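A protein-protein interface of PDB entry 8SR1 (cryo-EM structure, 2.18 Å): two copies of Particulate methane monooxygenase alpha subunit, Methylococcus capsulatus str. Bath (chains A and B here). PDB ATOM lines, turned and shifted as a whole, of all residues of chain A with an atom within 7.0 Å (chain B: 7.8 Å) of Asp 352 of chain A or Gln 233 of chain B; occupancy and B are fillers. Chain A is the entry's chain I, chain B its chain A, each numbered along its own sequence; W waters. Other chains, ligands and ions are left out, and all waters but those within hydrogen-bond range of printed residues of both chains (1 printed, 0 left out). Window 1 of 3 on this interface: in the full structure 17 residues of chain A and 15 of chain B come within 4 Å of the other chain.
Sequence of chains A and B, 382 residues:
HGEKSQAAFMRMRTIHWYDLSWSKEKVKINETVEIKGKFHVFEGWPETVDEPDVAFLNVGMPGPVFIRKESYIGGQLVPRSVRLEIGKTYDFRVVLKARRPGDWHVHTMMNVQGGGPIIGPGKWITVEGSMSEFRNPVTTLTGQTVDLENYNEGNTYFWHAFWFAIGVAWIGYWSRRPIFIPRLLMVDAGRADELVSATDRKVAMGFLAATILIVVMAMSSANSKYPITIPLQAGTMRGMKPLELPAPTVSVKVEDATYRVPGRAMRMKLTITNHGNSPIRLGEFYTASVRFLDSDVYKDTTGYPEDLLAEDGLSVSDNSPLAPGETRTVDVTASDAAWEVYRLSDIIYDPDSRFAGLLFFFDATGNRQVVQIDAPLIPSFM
Glu 47 of chain A touches Gly 235 of chain B.
O of Ile 348 of chain A touches CG2 of Ile 230 of chain B (3.9 Å).
Ile 348 of chain A touches Pro 231 of chain B.
Tyr 349 of chain A touches Pro 231 of chain B (O to CG, 3.2 Å).
Pro 231 of chain B touches Pro 351 of chain A.
Pro 351 of chain A touches Gln 233 of chain B (O to CA, 3.2 Å).
O of Ala 234 of chain B touches CB of Asp 352 of chain A, at 3.8 Å.
Arg 354 of chain A touches Arg 80 of chain B (NH2 to NH1, 3.6 Å).
Arg 354 of chain A touches Thr 236 of chain B.
Arg 354 of chain A touches Met 237 of chain B (NH1 to CG, 3.4 Å).
Asp 352 of chain A touches just these residues of chain B: Arg 80 (2.5 Å), Gln 233 (3.7 Å) and Ala 234 (3.8 Å).
Of the printed residues of chain A, Gln 233 of chain B touches Asp 350, Pro 351, Asp 352 and Ser 353.
Printed residues of chain A within 4 Å of Ala 234 of chain B: Pro 351 (3.0 Å) and Asp 352 (3.8 Å).
Of the printed residues of chain B, Ile 348 of chain A touches Ile 230 and Pro 231.
Printed residues of chain B within 4 Å of Glu 47 of chain A: Gly 235 (3.7 Å) and Thr 236 (3.1 Å).
Of the printed residues of chain B, Ser 353 of chain A touches Gln 233.
Of the printed residues of chain B, Asp 350 of chain A touches Pro 231 (3.4 Å) and Gln 233 (3.3 Å).
Pro 79 of chain B touches none of the printed residues of chain A.
The nearest residue of chain B that does not touch Asp 352 of chain A is Gly 235 of chain B (4.8 Å).
The nearest residue of chain A that does not touch Gln 233 of chain B is Arg 354 of chain A (5.8 Å).
The nearest printed residue of chain A that does not touch Pro 231 of chain B is Asp 352 of chain A (6.0 Å).
Water W1 lies within hydrogen-bond range of the backbone carbonyl oxygen (O) of Thr 236 of chain B (2.8 Å) and the backbone NH (N) of Glu 47 of chain A (3.1 Å).
Along chain B the printed residues that touch a printed residue of chain A span positions 80 to 237.
Printed residues of chain A that touch a printed residue of chain B: Glu 47, Ile 348, Tyr 349, Asp 350, Pro 351, Asp 352, Ser 353 and Arg 354.
Among the printed residues, Asp or Glu carboxylates within 4 Å of a Lys or Arg side-chain nitrogen of the other chain: Asp 352 of chain A with Arg 80 of chain B.
The guanidinium group of Arg 80 of chain B is in hydrogen-bond range of the backbone carbonyl oxygen of Ala 234 of chain B, 3.4 Å away.
NH1 of Arg 80 of chain B is in hydrogen-bond range of O of Gly 235 of chain B, 3.1 Å away.
The side-chain amide nitrogen of Gln 233 of chain B is in hydrogen-bond range of the backbone carbonyl oxygen of Pro 231 of chain B (3.0 Å).
N of Ala 8 of chain A is in hydrogen-bond range of OD2 of Asp 350 of chain A (3.1 Å).
The side-chain carboxylate (OD2) of Asp 350 of chain A is in hydrogen-bond range of the backbone NH (N) of Phe 9 of chain A, at 3.1 Å.
The backbone carbonyl oxygen of Leu 377 of chain A lies within hydrogen-bond range of the side-chain hydroxyl of Ser 353 of chain A, 2.7 Å away.
The guanidinium group (NH2) of Arg 80 of chain B is in salt-bridge range of the side-chain carboxylate (OD1) of Asp 352 of chain A (2.5 Å).
NE2 of Gln 233 of chain B sits at hydrogen-bond distance from O of Asp 350 of chain A (3.3 Å).
The side-chain amide oxygen (OE1) of Gln 233 of chain B lies within hydrogen-bond range of the backbone NH (N) of Ser 353 of chain A (3.0 Å).
The backbone NH (N) of Ala 234 of chain B sits at hydrogen-bond distance from the backbone carbonyl oxygen (O) of Pro 351 of chain A (3.0 Å).
The side-chain hydroxyl (OG1) of Thr 236 of chain B sits close to the side-chain carboxylate (OE1) of Glu 47 of chain A, at 3.1 Å.
No position is printed for both chains.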
ATOM      1  N   ALA A   8     -24.964  -0.858 -11.404  1.00  0.00           N
ATOM      2  CA  ALA A   8     -25.121  -1.658 -10.195  1.00  0.00           C
ATOM      3  C   ALA A   8     -25.736  -0.845  -9.065  1.00  0.00           C
ATOM      4  O   ALA A   8     -26.625  -1.331  -8.356  1.00  0.00           O
ATOM      5  CB  ALA A   8     -23.770  -2.235  -9.769  1.00  0.00           C
ATOM      6  N   PHE A   9     -25.283   0.398  -8.879  1.00  0.00           N
ATOM      7  CA  PHE A   9     -25.814   1.204  -7.786  1.00  0.00           C
ATOM      8  C   PHE A   9     -27.263   1.593  -8.045  1.00  0.00           C
ATOM      9  O   PHE A   9     -28.050   1.742  -7.103  1.00  0.00           O
ATOM     10  CB  PHE A   9     -24.938   2.437  -7.559  1.00  0.00           C
ATOM     11  CG  PHE A   9     -25.269   3.613  -8.440  1.00  0.00           C
ATOM     12  CD1 PHE A   9     -24.721   3.720  -9.705  1.00  0.00           C
ATOM     13  CD2 PHE A   9     -26.094   4.630  -7.988  1.00  0.00           C
ATOM     14  CE1 PHE A   9     -25.005   4.805 -10.511  1.00  0.00           C
ATOM     15  CE2 PHE A   9     -26.386   5.716  -8.790  1.00  0.00           C
ATOM     16  CZ  PHE A   9     -25.835   5.806 -10.053  1.00  0.00           C
ATOM     17  N   MET A  10     -27.637   1.754  -9.314  1.00  0.00           N
ATOM     18  CA  MET A  10     -29.024   2.085  -9.625  1.00  0.00           C
ATOM     19  C   MET A  10     -29.931   0.879  -9.414  1.00  0.00           C
ATOM     20  O   MET A  10     -31.075   1.027  -8.972  1.00  0.00           O
ATOM     21  CB  MET A  10     -29.128   2.600 -11.057  1.00  0.00           C
ATOM     22  CG  MET A  10     -28.196   3.757 -11.311  1.00  0.00           C
ATOM     23  SD  MET A  10     -29.001   5.360 -11.376  1.00  0.00           S
ATOM     24  CE  MET A  10     -30.291   5.013 -12.548  1.00  0.00           C
ATOM     25  N   ARG A  13     -30.230   0.739  -5.469  1.00  0.00           N
ATOM     26  CA  ARG A  13     -31.070   1.744  -4.834  1.00  0.00           C
ATOM     27  C   ARG A  13     -32.082   2.287  -5.837  1.00  0.00           C
ATOM     28  O   ARG A  13     -31.981   3.422  -6.300  1.00  0.00           O
ATOM     29  CB  ARG A  13     -30.179   2.873  -4.298  1.00  0.00           C
ATOM     30  CG  ARG A  13     -28.779   2.435  -3.907  1.00  0.00           C
ATOM     31  CD  ARG A  13     -27.761   3.549  -4.103  1.00  0.00           C
ATOM     32  NE  ARG A  13     -28.140   4.790  -3.437  1.00  0.00           N
ATOM     33  CZ  ARG A  13     -27.943   5.043  -2.151  1.00  0.00           C
ATOM     34  NH1 ARG A  13     -27.370   4.160  -1.352  1.00  0.00           N
ATOM     35  NH2 ARG A  13     -28.327   6.215  -1.658  1.00  0.00           N
ATOM     36  N   PRO A  46     -32.252   7.763  -6.526  1.00  0.00           N
ATOM     37  CA  PRO A  46     -31.233   8.544  -7.240  1.00  0.00           C
ATOM     38  C   PRO A  46     -31.846   9.743  -7.946  1.00  0.00           C
ATOM     39  O   PRO A  46     -32.941   9.663  -8.508  1.00  0.00           O
ATOM     40  CB  PRO A  46     -30.644   7.536  -8.234  1.00  0.00           C
ATOM     41  CG  PRO A  46     -31.687   6.484  -8.381  1.00  0.00           C
ATOM     42  CD  PRO A  46     -32.398   6.403  -7.069  1.00  0.00           C
ATOM     43  N   GLU A  47     -31.124  10.865  -7.914  1.00  0.00           N
ATOM     44  CA  GLU A  47     -31.628  12.091  -8.526  1.00  0.00           C
ATOM     45  C   GLU A  47     -31.744  11.974 -10.038  1.00  0.00           C
ATOM     46  O   GLU A  47     -32.555  12.681 -10.645  1.00  0.00           O
ATOM     47  CB  GLU A  47     -30.727  13.270  -8.158  1.00  0.00           C
ATOM     48  CG  GLU A  47     -29.417  13.326  -8.928  1.00  0.00           C
ATOM     49  CD  GLU A  47     -28.965  14.747  -9.200  1.00  0.00           C
ATOM     50  OE1 GLU A  47     -29.833  15.626  -9.365  1.00  0.00           O
ATOM     51  OE2 GLU A  47     -27.739  14.983  -9.244  1.00  0.00           O
ATOM     52  N   ILE A 347     -19.873  -1.920  -9.968  1.00  0.00           N
ATOM     53  CA  ILE A 347     -20.177  -0.612  -9.313  1.00  0.00           C
ATOM     54  C   ILE A 347     -18.886   0.222  -9.334  1.00  0.00           C
ATOM     55  O   ILE A 347     -18.963   1.445  -9.109  1.00  0.00           O
ATOM     56  CB  ILE A 347     -20.769  -0.830  -7.903  1.00  0.00           C
ATOM     57  CG1 ILE A 347     -21.305   0.465  -7.279  1.00  0.00           C
ATOM     58  CG2 ILE A 347     -19.775  -1.531  -6.994  1.00  0.00           C
ATOM     59  CD1 ILE A 347     -22.086   0.260  -6.007  1.00  0.00           C
ATOM     60  N   ILE A 348     -17.741  -0.400  -9.645  1.00  0.00           N
ATOM     61  CA  ILE A 348     -16.517   0.382  -9.770  1.00  0.00           C
ATOM     62  C   ILE A 348     -16.578   1.295 -10.989  1.00  0.00           C
ATOM     63  O   ILE A 348     -15.911   2.337 -11.029  1.00  0.00           O
ATOM     64  CB  ILE A 348     -15.293  -0.552  -9.812  1.00  0.00           C
ATOM     65  CG1 ILE A 348     -14.008   0.230  -9.536  1.00  0.00           C
ATOM     66  CG2 ILE A 348     -15.217  -1.293 -11.143  1.00  0.00           C
ATOM     67  CD1 ILE A 348     -12.752  -0.545  -9.843  1.00  0.00           C
ATOM     68  N   TYR A 349     -17.371   0.930 -11.995  1.00  0.00           N
ATOM     69  CA  TYR A 349     -17.580   1.776 -13.163  1.00  0.00           C
ATOM     70  C   TYR A 349     -18.611   2.870 -12.919  1.00  0.00           C
ATOM     71  O   TYR A 349     -18.673   3.828 -13.696  1.00  0.00           O
ATOM     72  CB  TYR A 349     -18.008   0.908 -14.353  1.00  0.00           C
ATOM     73  CG  TYR A 349     -18.157   1.652 -15.661  1.00  0.00           C
ATOM     74  CD1 TYR A 349     -17.062   1.877 -16.481  1.00  0.00           C
ATOM     75  CD2 TYR A 349     -19.396   2.126 -16.076  1.00  0.00           C
ATOM     76  CE1 TYR A 349     -17.193   2.553 -17.676  1.00  0.00           C
ATOM     77  CE2 TYR A 349     -19.536   2.806 -17.268  1.00  0.00           C
ATOM     78  CZ  TYR A 349     -18.432   3.021 -18.062  1.00  0.00           C
ATOM     79  OH  TYR A 349     -18.565   3.693 -19.252  1.00  0.00           O
ATOM     80  N   ASP A 350     -19.396   2.765 -11.858  1.00  0.00           N
ATOM     81  CA  ASP A 350     -20.498   3.682 -11.628  1.00  0.00           C
ATOM     82  C   ASP A 350     -20.008   5.027 -11.096  1.00  0.00           C
ATOM     83  O   ASP A 350     -19.004   5.094 -10.383  1.00  0.00           O
ATOM     84  CB  ASP A 350     -21.489   3.074 -10.644  1.00  0.00           C
ATOM     85  CG  ASP A 350     -22.307   1.955 -11.258  1.00  0.00           C
ATOM     86  OD1 ASP A 350     -22.479   1.951 -12.495  1.00  0.00           O
ATOM     87  OD2 ASP A 350     -22.783   1.078 -10.504  1.00  0.00           O
ATOM     88  N   PRO A 351     -20.705   6.113 -11.429  1.00  0.00           N
ATOM     89  CA  PRO A 351     -20.366   7.428 -10.875  1.00  0.00           C
ATOM     90  C   PRO A 351     -20.921   7.688  -9.482  1.00  0.00           C
ATOM     91  O   PRO A 351     -20.825   8.822  -9.004  1.00  0.00           O
ATOM     92  CB  PRO A 351     -20.996   8.388 -11.895  1.00  0.00           C
ATOM     93  CG  PRO A 351     -22.178   7.649 -12.396  1.00  0.00           C
ATOM     94  CD  PRO A 351     -21.784   6.198 -12.428  1.00  0.00           C
ATOM     95  N   ASP A 352     -21.504   6.684  -8.828  1.00  0.00           N
ATOM     96  CA  ASP A 352     -22.023   6.845  -7.470  1.00  0.00           C
ATOM     97  C   ASP A 352     -21.852   5.502  -6.766  1.00  0.00           C
ATOM     98  O   ASP A 352     -22.709   4.625  -6.887  1.00  0.00           O
ATOM     99  CB  ASP A 352     -23.478   7.293  -7.482  1.00  0.00           C
ATOM    100  CG  ASP A 352     -23.958   7.762  -6.125  1.00  0.00           C
ATOM    101  OD1 ASP A 352     -23.195   7.649  -5.142  1.00  0.00           O
ATOM    102  OD2 ASP A 352     -25.106   8.242  -6.035  1.00  0.00           O
ATOM    103  N   SER A 353     -20.751   5.355  -6.030  1.00  0.00           N
ATOM    104  CA  SER A 353     -20.423   4.088  -5.375  1.00  0.00           C
ATOM    105  C   SER A 353     -21.093   4.025  -4.002  1.00  0.00           C
ATOM    106  O   SER A 353     -20.459   4.094  -2.947  1.00  0.00           O
ATOM    107  CB  SER A 353     -18.917   3.916  -5.270  1.00  0.00           C
ATOM    108  OG  SER A 353     -18.570   2.547  -5.151  1.00  0.00           O
ATOM    109  N   ARG A 354     -22.414   3.892  -4.036  1.00  0.00           N
ATOM    110  CA  ARG A 354     -23.212   3.687  -2.841  1.00  0.00           C
ATOM    111  C   ARG A 354     -24.145   2.511  -3.071  1.00  0.00           C
ATOM    112  O   ARG A 354     -24.703   2.343  -4.160  1.00  0.00           O
ATOM    113  CB  ARG A 354     -24.016   4.940  -2.473  1.00  0.00           C
ATOM    114  CG  ARG A 354     -23.172   6.076  -1.923  1.00  0.00           C
ATOM    115  CD  ARG A 354     -24.030   7.260  -1.518  1.00  0.00           C
ATOM    116  NE  ARG A 354     -24.778   7.806  -2.644  1.00  0.00           N
ATOM    117  CZ  ARG A 354     -25.823   8.614  -2.523  1.00  0.00           C
ATOM    118  NH1 ARG A 354     -26.268   8.998  -1.341  1.00  0.00           N
ATOM    119  NH2 ARG A 354     -26.437   9.047  -3.623  1.00  0.00           N
ATOM    120  N   PHE A 355     -24.301   1.687  -2.044  1.00  0.00           N
ATOM    121  CA  PHE A 355     -25.158   0.519  -2.116  1.00  0.00           C
ATOM    122  C   PHE A 355     -26.339   0.683  -1.171  1.00  0.00           C
ATOM    123  O   PHE A 355     -26.304   1.476  -0.228  1.00  0.00           O
ATOM    124  CB  PHE A 355     -24.386  -0.768  -1.776  1.00  0.00           C
ATOM    125  CG  PHE A 355     -24.395  -1.113  -0.313  1.00  0.00           C
ATOM    126  CD1 PHE A 355     -23.468  -0.552   0.547  1.00  0.00           C
ATOM    127  CD2 PHE A 355     -25.318  -2.013   0.200  1.00  0.00           C
ATOM    128  CE1 PHE A 355     -23.468  -0.865   1.891  1.00  0.00           C
ATOM    129  CE2 PHE A 355     -25.327  -2.327   1.545  1.00  0.00           C
ATOM    130  CZ  PHE A 355     -24.397  -1.757   2.391  1.00  0.00           C
ATOM    131  N   LEU A 377     -19.921   2.279  -0.790  1.00  0.00           N
ATOM    132  CA  LEU A 377     -19.275   0.995  -1.034  1.00  0.00           C
ATOM    133  C   LEU A 377     -17.884   1.281  -1.589  1.00  0.00           C
ATOM    134  O   LEU A 377     -17.746   1.750  -2.724  1.00  0.00           O
ATOM    135  CB  LEU A 377     -20.104   0.147  -1.994  1.00  0.00           C
ATOM    136  CG  LEU A 377     -19.683  -1.311  -2.181  1.00  0.00           C
ATOM    137  CD1 LEU A 377     -19.883  -2.099  -0.898  1.00  0.00           C
ATOM    138  CD2 LEU A 377     -20.453  -1.943  -3.330  1.00  0.00           C
ATOM    139  N   PRO B  79     -20.145  15.773   0.427  1.00  0.00           N
ATOM    140  CA  PRO B  79     -19.346  16.361  -0.658  1.00  0.00           C
ATOM    141  C   PRO B  79     -20.148  16.642  -1.916  1.00  0.00           C
ATOM    142  O   PRO B  79     -19.627  17.309  -2.820  1.00  0.00           O
ATOM    143  CB  PRO B  79     -18.274  15.299  -0.915  1.00  0.00           C
ATOM    144  CG  PRO B  79     -18.948  14.023  -0.565  1.00  0.00           C
ATOM    145  CD  PRO B  79     -19.899  14.328   0.566  1.00  0.00           C
ATOM    146  N   ARG B  80     -21.379  16.162  -2.003  1.00  0.00           N
ATOM    147  CA  ARG B  80     -22.242  16.361  -3.154  1.00  0.00           C
ATOM    148  C   ARG B  80     -23.458  17.185  -2.746  1.00  0.00           C
ATOM    149  O   ARG B  80     -23.629  17.557  -1.581  1.00  0.00           O
ATOM    150  CB  ARG B  80     -22.662  15.017  -3.749  1.00  0.00           C
ATOM    151  CG  ARG B  80     -21.549  13.982  -3.787  1.00  0.00           C
ATOM    152  CD  ARG B  80     -21.771  12.984  -4.901  1.00  0.00           C
ATOM    153  NE  ARG B  80     -21.363  11.634  -4.531  1.00  0.00           N
ATOM    154  CZ  ARG B  80     -22.170  10.582  -4.540  1.00  0.00           C
ATOM    155  NH1 ARG B  80     -23.443  10.691  -4.873  1.00  0.00           N
ATOM    156  NH2 ARG B  80     -21.681   9.390  -4.212  1.00  0.00           N
ATOM    157  N   ILE B 230     -11.522   5.534 -11.473  1.00  0.00           N
ATOM    158  CA  ILE B 230     -12.969   5.569 -11.279  1.00  0.00           C
ATOM    159  C   ILE B 230     -13.504   6.849 -11.912  1.00  0.00           C
ATOM    160  O   ILE B 230     -12.773   7.844 -12.001  1.00  0.00           O
ATOM    161  CB  ILE B 230     -13.340   5.486  -9.790  1.00  0.00           C
ATOM    162  CG1 ILE B 230     -12.671   6.617  -9.005  1.00  0.00           C
ATOM    163  CG2 ILE B 230     -12.959   4.131  -9.213  1.00  0.00           C
ATOM    164  CD1 ILE B 230     -13.433   7.030  -7.770  1.00  0.00           C
ATOM    165  N   PRO B 231     -14.752   6.871 -12.366  1.00  0.00           N
ATOM    166  CA  PRO B 231     -15.321   8.113 -12.893  1.00  0.00           C
ATOM    167  C   PRO B 231     -15.560   9.120 -11.777  1.00  0.00           C
ATOM    168  O   PRO B 231     -15.472   8.814 -10.587  1.00  0.00           O
ATOM    169  CB  PRO B 231     -16.636   7.664 -13.533  1.00  0.00           C
ATOM    170  CG  PRO B 231     -17.000   6.427 -12.793  1.00  0.00           C
ATOM    171  CD  PRO B 231     -15.706   5.752 -12.446  1.00  0.00           C
ATOM    172  N   LEU B 232     -15.860  10.349 -12.189  1.00  0.00           N
ATOM    173  CA  LEU B 232     -16.205  11.391 -11.235  1.00  0.00           C
ATOM    174  C   LEU B 232     -17.439  10.982 -10.440  1.00  0.00           C
ATOM    175  O   LEU B 232     -18.430  10.516 -11.007  1.00  0.00           O
ATOM    176  CB  LEU B 232     -16.451  12.709 -11.962  1.00  0.00           C
ATOM    177  CG  LEU B 232     -15.235  13.304 -12.669  1.00  0.00           C
ATOM    178  CD1 LEU B 232     -15.639  14.480 -13.536  1.00  0.00           C
ATOM    179  CD2 LEU B 232     -14.191  13.721 -11.654  1.00  0.00           C
ATOM    180  N   GLN B 233     -17.372  11.152  -9.124  1.00  0.00           N
ATOM    181  CA  GLN B 233     -18.460  10.761  -8.240  1.00  0.00           C
ATOM    182  C   GLN B 233     -19.414  11.938  -8.068  1.00  0.00           C
ATOM    183  O   GLN B 233     -19.037  12.969  -7.502  1.00  0.00           O
ATOM    184  CB  GLN B 233     -17.916  10.297  -6.889  1.00  0.00           C
ATOM    185  CG  GLN B 233     -17.003   9.085  -6.976  1.00  0.00           C
ATOM    186  CD  GLN B 233     -17.713   7.850  -7.487  1.00  0.00           C
ATOM    187  OE1 GLN B 233     -18.396   7.157  -6.735  1.00  0.00           O
ATOM    188  NE2 GLN B 233     -17.551   7.562  -8.773  1.00  0.00           N
ATOM    189  N   ALA B 234     -20.642  11.778  -8.551  1.00  0.00           N
ATOM    190  CA  ALA B 234     -21.622  12.851  -8.525  1.00  0.00           C
ATOM    191  C   ALA B 234     -22.992  12.267  -8.216  1.00  0.00           C
ATOM    192  O   ALA B 234     -23.196  11.051  -8.245  1.00  0.00           O
ATOM    193  CB  ALA B 234     -21.641  13.620  -9.848  1.00  0.00           C
ATOM    194  N   GLY B 235     -23.931  13.155  -7.907  1.00  0.00           N
ATOM    195  CA  GLY B 235     -25.295  12.750  -7.633  1.00  0.00           C
ATOM    196  C   GLY B 235     -25.832  13.311  -6.332  1.00  0.00           C
ATOM    197  O   GLY B 235     -25.174  13.216  -5.293  1.00  0.00           O
ATOM    198  N   THR B 236     -27.023  13.904  -6.382  1.00  0.00           N
ATOM    199  CA  THR B 236     -27.640  14.445  -5.178  1.00  0.00           C
ATOM    200  C   THR B 236     -27.869  13.340  -4.156  1.00  0.00           C
ATOM    201  O   THR B 236     -28.280  12.227  -4.497  1.00  0.00           O
ATOM    202  CB  THR B 236     -28.966  15.131  -5.524  1.00  0.00           C
ATOM    203  OG1 THR B 236     -28.730  16.170  -6.480  1.00  0.00           O
ATOM    204  CG2 THR B 236     -29.602  15.736  -4.280  1.00  0.00           C
ATOM    205  N   MET B 237     -27.594  13.651  -2.895  1.00  0.00           N
ATOM    206  CA  MET B 237     -27.686  12.685  -1.809  1.00  0.00           C
ATOM    207  C   MET B 237     -28.967  12.939  -1.024  1.00  0.00           C
ATOM    208  O   MET B 237     -29.181  14.042  -0.511  1.00  0.00           O
ATOM    209  CB  MET B 237     -26.463  12.787  -0.902  1.00  0.00           C
ATOM    210  CG  MET B 237     -25.207  12.189  -1.515  1.00  0.00           C
ATOM    211  SD  MET B 237     -23.715  12.590  -0.590  1.00  0.00           S
ATOM    212  CE  MET B 237     -24.191  12.049   1.043  1.00  0.00           C
HETATM  213  O   HOH W   1     -28.496  10.215  -6.374  1.00  0.00           O
